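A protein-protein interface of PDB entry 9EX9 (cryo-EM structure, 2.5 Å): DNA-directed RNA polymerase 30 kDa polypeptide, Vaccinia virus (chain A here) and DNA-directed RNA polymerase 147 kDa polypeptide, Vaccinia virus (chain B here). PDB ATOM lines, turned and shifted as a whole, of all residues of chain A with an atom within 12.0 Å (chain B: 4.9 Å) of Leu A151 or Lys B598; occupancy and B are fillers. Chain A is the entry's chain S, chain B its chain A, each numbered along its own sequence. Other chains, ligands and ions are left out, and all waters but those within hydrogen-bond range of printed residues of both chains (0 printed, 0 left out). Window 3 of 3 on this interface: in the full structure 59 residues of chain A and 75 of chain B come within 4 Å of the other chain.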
ATOM      1  N   TYR A 144     -24.557 -25.652   2.593  1.00  0.00           N
ATOM      2  CA  TYR A 144     -24.340 -25.413   1.175  1.00  0.00           C
ATOM      3  C   TYR A 144     -24.606 -23.972   0.765  1.00  0.00           C
ATOM      4  O   TYR A 144     -24.377 -23.624  -0.398  1.00  0.00           O
ATOM      5  CB  TYR A 144     -25.216 -26.358   0.351  1.00  0.00           C
ATOM      6  CG  TYR A 144     -24.943 -27.815   0.635  1.00  0.00           C
ATOM      7  CD1 TYR A 144     -23.931 -28.491  -0.026  1.00  0.00           C
ATOM      8  CD2 TYR A 144     -25.691 -28.512   1.569  1.00  0.00           C
ATOM      9  CE1 TYR A 144     -23.676 -29.819   0.234  1.00  0.00           C
ATOM     10  CE2 TYR A 144     -25.443 -29.840   1.832  1.00  0.00           C
ATOM     11  CZ  TYR A 144     -24.435 -30.488   1.162  1.00  0.00           C
ATOM     12  OH  TYR A 144     -24.184 -31.814   1.423  1.00  0.00           O
ATOM     13  N   ASN A 145     -25.071 -23.125   1.684  1.00  0.00           N
ATOM     14  CA  ASN A 145     -25.293 -21.723   1.352  1.00  0.00           C
ATOM     15  C   ASN A 145     -24.001 -21.013   0.985  1.00  0.00           C
ATOM     16  O   ASN A 145     -24.046 -19.929   0.397  1.00  0.00           O
ATOM     17  CB  ASN A 145     -25.968 -21.008   2.520  1.00  0.00           C
ATOM     18  CG  ASN A 145     -27.346 -21.556   2.817  1.00  0.00           C
ATOM     19  OD1 ASN A 145     -27.706 -22.638   2.357  1.00  0.00           O
ATOM     20  ND2 ASN A 145     -28.126 -20.811   3.589  1.00  0.00           N
ATOM     21  N   ASP A 146     -22.850 -21.592   1.322  1.00  0.00           N
ATOM     22  CA  ASP A 146     -21.581 -21.017   0.902  1.00  0.00           C
ATOM     23  C   ASP A 146     -21.390 -21.094  -0.606  1.00  0.00           C
ATOM     24  O   ASP A 146     -20.574 -20.346  -1.152  1.00  0.00           O
ATOM     25  CB  ASP A 146     -20.430 -21.729   1.610  1.00  0.00           C
ATOM     26  CG  ASP A 146     -20.657 -21.852   3.101  1.00  0.00           C
ATOM     27  OD1 ASP A 146     -21.667 -21.304   3.590  1.00  0.00           O
ATOM     28  OD2 ASP A 146     -19.836 -22.500   3.781  1.00  0.00           O
ATOM     29  N   TYR A 147     -22.114 -21.983  -1.285  1.00  0.00           N
ATOM     30  CA  TYR A 147     -22.021 -22.099  -2.735  1.00  0.00           C
ATOM     31  C   TYR A 147     -23.101 -21.311  -3.456  1.00  0.00           C
ATOM     32  O   TYR A 147     -22.861 -20.817  -4.561  1.00  0.00           O
ATOM     33  CB  TYR A 147     -22.125 -23.566  -3.160  1.00  0.00           C
ATOM     34  CG  TYR A 147     -21.021 -24.453  -2.645  1.00  0.00           C
ATOM     35  CD1 TYR A 147     -19.823 -24.566  -3.328  1.00  0.00           C
ATOM     36  CD2 TYR A 147     -21.184 -25.186  -1.482  1.00  0.00           C
ATOM     37  CE1 TYR A 147     -18.816 -25.376  -2.866  1.00  0.00           C
ATOM     38  CE2 TYR A 147     -20.182 -25.999  -1.012  1.00  0.00           C
ATOM     39  CZ  TYR A 147     -18.999 -26.091  -1.708  1.00  0.00           C
ATOM     40  OH  TYR A 147     -17.991 -26.902  -1.244  1.00  0.00           O
ATOM     41  N   PHE A 148     -24.286 -21.190  -2.863  1.00  0.00           N
ATOM     42  CA  PHE A 148     -25.439 -20.611  -3.535  1.00  0.00           C
ATOM     43  C   PHE A 148     -25.840 -19.263  -2.949  1.00  0.00           C
ATOM     44  O   PHE A 148     -26.998 -18.857  -3.075  1.00  0.00           O
ATOM     45  CB  PHE A 148     -26.610 -21.590  -3.479  1.00  0.00           C
ATOM     46  CG  PHE A 148     -26.276 -22.956  -4.000  1.00  0.00           C
ATOM     47  CD1 PHE A 148     -26.237 -23.202  -5.359  1.00  0.00           C
ATOM     48  CD2 PHE A 148     -25.993 -23.991  -3.133  1.00  0.00           C
ATOM     49  CE1 PHE A 148     -25.925 -24.453  -5.840  1.00  0.00           C
ATOM     50  CE2 PHE A 148     -25.682 -25.246  -3.611  1.00  0.00           C
ATOM     51  CZ  PHE A 148     -25.647 -25.474  -4.965  1.00  0.00           C
ATOM     52  N   ASN A 149     -24.910 -18.560  -2.311  1.00  0.00           N
ATOM     53  CA  ASN A 149     -25.182 -17.226  -1.795  1.00  0.00           C
ATOM     54  C   ASN A 149     -24.882 -16.128  -2.802  1.00  0.00           C
ATOM     55  O   ASN A 149     -25.252 -14.975  -2.561  1.00  0.00           O
ATOM     56  CB  ASN A 149     -24.368 -16.972  -0.525  1.00  0.00           C
ATOM     57  CG  ASN A 149     -25.219 -16.998   0.728  1.00  0.00           C
ATOM     58  OD1 ASN A 149     -26.365 -17.448   0.708  1.00  0.00           O
ATOM     59  ND2 ASN A 149     -24.660 -16.512   1.829  1.00  0.00           N
ATOM     60  N   VAL A 150     -24.224 -16.451  -3.915  1.00  0.00           N
ATOM     61  CA  VAL A 150     -23.939 -15.442  -4.924  1.00  0.00           C
ATOM     62  C   VAL A 150     -25.238 -14.800  -5.374  1.00  0.00           C
ATOM     63  O   VAL A 150     -26.262 -15.473  -5.545  1.00  0.00           O
ATOM     64  CB  VAL A 150     -23.189 -16.067  -6.111  1.00  0.00           C
ATOM     65  CG1 VAL A 150     -23.057 -15.064  -7.240  1.00  0.00           C
ATOM     66  CG2 VAL A 150     -21.826 -16.560  -5.673  1.00  0.00           C
ATOM     67  N   LEU A 151     -25.206 -13.486  -5.560  1.00  0.00           N
ATOM     68  CA  LEU A 151     -26.376 -12.762  -6.028  1.00  0.00           C
ATOM     69  C   LEU A 151     -27.547 -12.959  -5.072  1.00  0.00           C
ATOM     70  O   LEU A 151     -27.582 -12.371  -3.992  1.00  0.00           O
ATOM     71  CB  LEU A 151     -26.756 -13.223  -7.438  1.00  0.00           C
ATOM     72  CG  LEU A 151     -28.059 -12.664  -8.006  1.00  0.00           C
ATOM     73  CD1 LEU A 151     -28.056 -11.145  -7.987  1.00  0.00           C
ATOM     74  CD2 LEU A 151     -28.275 -13.180  -9.410  1.00  0.00           C
ATOM     75  N   ILE B 594     -25.751  -6.070 -17.119  1.00  0.00           N
ATOM     76  CA  ILE B 594     -25.982  -6.610 -15.782  1.00  0.00           C
ATOM     77  C   ILE B 594     -26.375  -8.078 -15.864  1.00  0.00           C
ATOM     78  O   ILE B 594     -25.866  -8.923 -15.116  1.00  0.00           O
ATOM     79  CB  ILE B 594     -27.047  -5.781 -15.047  1.00  0.00           C
ATOM     80  CG1 ILE B 594     -26.473  -4.411 -14.690  1.00  0.00           C
ATOM     81  CG2 ILE B 594     -27.529  -6.517 -13.809  1.00  0.00           C
ATOM     82  CD1 ILE B 594     -27.478  -3.453 -14.114  1.00  0.00           C
ATOM     83  N   ASN B 595     -27.299  -8.404 -16.769  1.00  0.00           N
ATOM     84  CA  ASN B 595     -27.713  -9.795 -16.918  1.00  0.00           C
ATOM     85  C   ASN B 595     -26.547 -10.677 -17.342  1.00  0.00           C
ATOM     86  O   ASN B 595     -26.375 -11.790 -16.825  1.00  0.00           O
ATOM     87  CB  ASN B 595     -28.849  -9.894 -17.933  1.00  0.00           C
ATOM     88  CG  ASN B 595     -30.182  -9.483 -17.357  1.00  0.00           C
ATOM     89  OD1 ASN B 595     -30.527  -9.846 -16.236  1.00  0.00           O
ATOM     90  ND2 ASN B 595     -30.947  -8.726 -18.129  1.00  0.00           N
ATOM     91  N   VAL B 596     -25.738 -10.199 -18.291  1.00  0.00           N
ATOM     92  CA  VAL B 596     -24.630 -11.004 -18.799  1.00  0.00           C
ATOM     93  C   VAL B 596     -23.641 -11.318 -17.686  1.00  0.00           C
ATOM     94  O   VAL B 596     -23.068 -12.411 -17.638  1.00  0.00           O
ATOM     95  CB  VAL B 596     -23.944 -10.290 -19.975  1.00  0.00           C
ATOM     96  CG1 VAL B 596     -22.632 -10.957 -20.301  1.00  0.00           C
ATOM     97  CG2 VAL B 596     -24.845 -10.297 -21.187  1.00  0.00           C
ATOM     98  N   GLU B 597     -23.406 -10.363 -16.789  1.00  0.00           N
ATOM     99  CA  GLU B 597     -22.500 -10.620 -15.672  1.00  0.00           C
ATOM    100  C   GLU B 597     -23.112 -11.592 -14.667  1.00  0.00           C
ATOM    101  O   GLU B 597     -22.456 -12.549 -14.224  1.00  0.00           O
ATOM    102  CB  GLU B 597     -22.140  -9.299 -14.998  1.00  0.00           C
ATOM    103  CG  GLU B 597     -21.429  -9.442 -13.673  1.00  0.00           C
ATOM    104  CD  GLU B 597     -21.058  -8.102 -13.081  1.00  0.00           C
ATOM    105  OE1 GLU B 597     -20.834  -7.153 -13.858  1.00  0.00           O
ATOM    106  OE2 GLU B 597     -21.000  -7.994 -11.840  1.00  0.00           O
ATOM    107  N   LYS B 598     -24.371 -11.364 -14.290  1.00  0.00           N
ATOM    108  CA  LYS B 598     -24.964 -12.154 -13.218  1.00  0.00           C
ATOM    109  C   LYS B 598     -25.131 -13.614 -13.614  1.00  0.00           C
ATOM    110  O   LYS B 598     -24.922 -14.514 -12.788  1.00  0.00           O
ATOM    111  CB  LYS B 598     -26.304 -11.553 -12.811  1.00  0.00           C
ATOM    112  CG  LYS B 598     -26.184 -10.193 -12.164  1.00  0.00           C
ATOM    113  CD  LYS B 598     -25.479 -10.276 -10.826  1.00  0.00           C
ATOM    114  CE  LYS B 598     -25.355  -8.913 -10.183  1.00  0.00           C
ATOM    115  NZ  LYS B 598     -24.447  -8.026 -10.953  1.00  0.00           N
ATOM    116  N   ILE B 599     -25.521 -13.883 -14.861  1.00  0.00           N
ATOM    117  CA  ILE B 599     -25.718 -15.274 -15.257  1.00  0.00           C
ATOM    118  C   ILE B 599     -24.404 -16.036 -15.159  1.00  0.00           C
ATOM    119  O   ILE B 599     -24.363 -17.186 -14.703  1.00  0.00           O
ATOM    120  CB  ILE B 599     -26.318 -15.353 -16.672  1.00  0.00           C
ATOM    121  CG1 ILE B 599     -26.787 -16.773 -16.978  1.00  0.00           C
ATOM    122  CG2 ILE B 599     -25.302 -14.920 -17.709  1.00  0.00           C
ATOM    123  CD1 ILE B 599     -27.849 -17.278 -16.042  1.00  0.00           C
ATOM    124  N   GLU B 600     -23.310 -15.406 -15.585  1.00  0.00           N
ATOM    125  CA  GLU B 600     -22.011 -16.060 -15.516  1.00  0.00           C
ATOM    126  C   GLU B 600     -21.591 -16.293 -14.072  1.00  0.00           C
ATOM    127  O   GLU B 600     -20.985 -17.321 -13.752  1.00  0.00           O
ATOM    128  CB  GLU B 600     -20.972 -15.227 -16.257  1.00  0.00           C
ATOM    129  CG  GLU B 600     -19.655 -15.937 -16.453  1.00  0.00           C
ATOM    130  CD  GLU B 600     -18.778 -15.263 -17.486  1.00  0.00           C
ATOM    131  OE1 GLU B 600     -19.213 -14.246 -18.065  1.00  0.00           O
ATOM    132  OE2 GLU B 600     -17.653 -15.752 -17.724  1.00  0.00           O
ATOM    133  N   LEU B 601     -21.904 -15.350 -13.181  1.00  0.00           N
ATOM    134  CA  LEU B 601     -21.610 -15.583 -11.769  1.00  0.00           C
ATOM    135  C   LEU B 601     -22.354 -16.810 -11.250  1.00  0.00           C
ATOM    136  O   LEU B 601     -21.781 -17.644 -10.533  1.00  0.00           O
ATOM    137  CB  LEU B 601     -21.974 -14.352 -10.943  1.00  0.00           C
ATOM    138  CG  LEU B 601     -20.802 -13.586 -10.334  1.00  0.00           C
ATOM    139  CD1 LEU B 601     -19.851 -13.104 -11.408  1.00  0.00           C
ATOM    140  CD2 LEU B 601     -21.322 -12.422  -9.525  1.00  0.00           C
ATOM    141  N   ILE B 602     -23.633 -16.937 -11.601  1.00  0.00           N
ATOM    142  CA  ILE B 602     -24.398 -18.103 -11.162  1.00  0.00           C
ATOM    143  C   ILE B 602     -23.771 -19.382 -11.699  1.00  0.00           C
ATOM    144  O   ILE B 602     -23.639 -20.384 -10.978  1.00  0.00           O
ATOM    145  CB  ILE B 602     -25.869 -17.977 -11.598  1.00  0.00           C
ATOM    146  CG1 ILE B 602     -26.536 -16.797 -10.896  1.00  0.00           C
ATOM    147  CG2 ILE B 602     -26.610 -19.268 -11.298  1.00  0.00           C
ATOM    148  CD1 ILE B 602     -27.904 -16.472 -11.432  1.00  0.00           C
ATOM    149  N   MET B 633     -31.445 -18.923  -7.069  1.00  0.00           N
ATOM    150  CA  MET B 633     -30.521 -17.966  -7.676  1.00  0.00           C
ATOM    151  C   MET B 633     -31.160 -17.274  -8.877  1.00  0.00           C
ATOM    152  O   MET B 633     -31.087 -16.042  -9.028  1.00  0.00           O
ATOM    153  CB  MET B 633     -29.228 -18.670  -8.078  1.00  0.00           C
ATOM    154  CG  MET B 633     -28.395 -19.130  -6.897  1.00  0.00           C
ATOM    155  SD  MET B 633     -26.715 -19.594  -7.343  1.00  0.00           S
ATOM    156  CE  MET B 633     -27.009 -21.094  -8.265  1.00  0.00           C
ATOM    157  N   ASN B 636     -33.706 -14.722  -7.810  1.00  0.00           N
ATOM    158  CA  ASN B 636     -33.063 -13.496  -7.359  1.00  0.00           C
ATOM    159  C   ASN B 636     -32.702 -12.614  -8.544  1.00  0.00           C
ATOM    160  O   ASN B 636     -32.904 -11.394  -8.505  1.00  0.00           O
ATOM    161  CB  ASN B 636     -31.822 -13.822  -6.532  1.00  0.00           C
ATOM    162  CG  ASN B 636     -32.161 -14.366  -5.165  1.00  0.00           C
ATOM    163  OD1 ASN B 636     -33.246 -14.128  -4.643  1.00  0.00           O
ATOM    164  ND2 ASN B 636     -31.230 -15.099  -4.572  1.00  0.00           N
ATOM    165  N   LEU B 637     -32.172 -13.212  -9.613  1.00  0.00           N
ATOM    166  CA  LEU B 637     -31.840 -12.405 -10.789  1.00  0.00           C
ATOM    167  C   LEU B 637     -33.086 -11.755 -11.388  1.00  0.00           C
ATOM    168  O   LEU B 637     -33.069 -10.576 -11.779  1.00  0.00           O
ATOM    169  CB  LEU B 637     -31.128 -13.259 -11.833  1.00  0.00           C
ATOM    170  CG  LEU B 637     -30.652 -12.515 -13.078  1.00  0.00           C
ATOM    171  CD1 LEU B 637     -29.745 -11.365 -12.705  1.00  0.00           C
ATOM    172  CD2 LEU B 637     -29.933 -13.460 -14.010  1.00  0.00           C
ATOM    173  N   LEU B 640     -34.093  -8.833  -9.371  1.00  0.00           N
ATOM    174  CA  LEU B 640     -33.191  -7.716  -9.633  1.00  0.00           C
ATOM    175  C   LEU B 640     -33.627  -6.946 -10.871  1.00  0.00           C
ATOM    176  O   LEU B 640     -33.663  -5.707 -10.868  1.00  0.00           O
ATOM    177  CB  LEU B 640     -31.767  -8.239  -9.793  1.00  0.00           C
ATOM    178  CG  LEU B 640     -30.699  -7.237 -10.217  1.00  0.00           C
ATOM    179  CD1 LEU B 640     -30.574  -6.127  -9.198  1.00  0.00           C
ATOM    180  CD2 LEU B 640     -29.379  -7.948 -10.395  1.00  0.00           C
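Among the printed residues, pairs that only touch across the chains: Phe A148 with Met B633 (3.7 Å), Val A150 with Leu B601 (3.9 Å), Leu A151 with Lys B598 (3.9 Å), Leu A151 with Ile B602 (3.9 Å) and Leu A151 with Leu B637 (3.7 Å).
Printed residues of chain B within 4 Å of Phe A148: Met B633. Of the printed residues of chain B, Val A150 touches Leu B601. Of the printed residues of chain B, Leu A151 touches Lys B598, Ile B602 and Leu B637. No residue of chain A comes within 4 Å of Ile B594. No residue of chain A comes within 4 Å of Val B596. No residue of chain A comes within 4 Å of Glu B597. Of the printed residues of chain A, Lys B598 touches Leu A151. No residue of chain A comes within 4 Å of Ile B599. Of chain A, only Val A150 (3.9 Å) comes within 4 Å of Leu B601. Ile B602 touches just one residue of chain A: Leu A151. No residue of chain A comes within 4 Å of Asn B636. The nearest residue of chain B that does not touch Leu A151 is Met B633 (4.03 Å). The nearest residue of chain A that does not touch Lys B598 is Val A150 (5.9 Å). The nearest printed residue of chain B that does not touch Phe A148 is Asn B636 (5.9 Å).
The side-chain carboxylate (OE2) of Glu B597 is in salt-bridge range of the side-chain amino group (NZ) of Lys B598, at 3.6 Å.
Printed residues of chain A that touch a printed residue of chain B: Phe A148, Val A150 and Leu A151. Hydrophobic or aromatic side chains of chain A within 4 Å of the printed part of chain B: Phe A148, Val A150 and Leu A151. Printed residues of chain B that touch a printed residue of chain A: Lys B598, Leu B601, Ile B602, Met B633 and Leu B637. Hydrophobic or aromatic side chains of chain B within 4 Å of the printed part of chain A: Leu B601, Ile B602, Met B633 and Leu B637. Along chain B the printed residues that touch a printed residue of chain A span positions 598 to 637. Among the printed residues, 5 pairs touch across the chains. Among the printed residues, no Asp or Glu carboxylate lies within 4 Å of a Lys or Arg side-chain nitrogen of the other chain.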
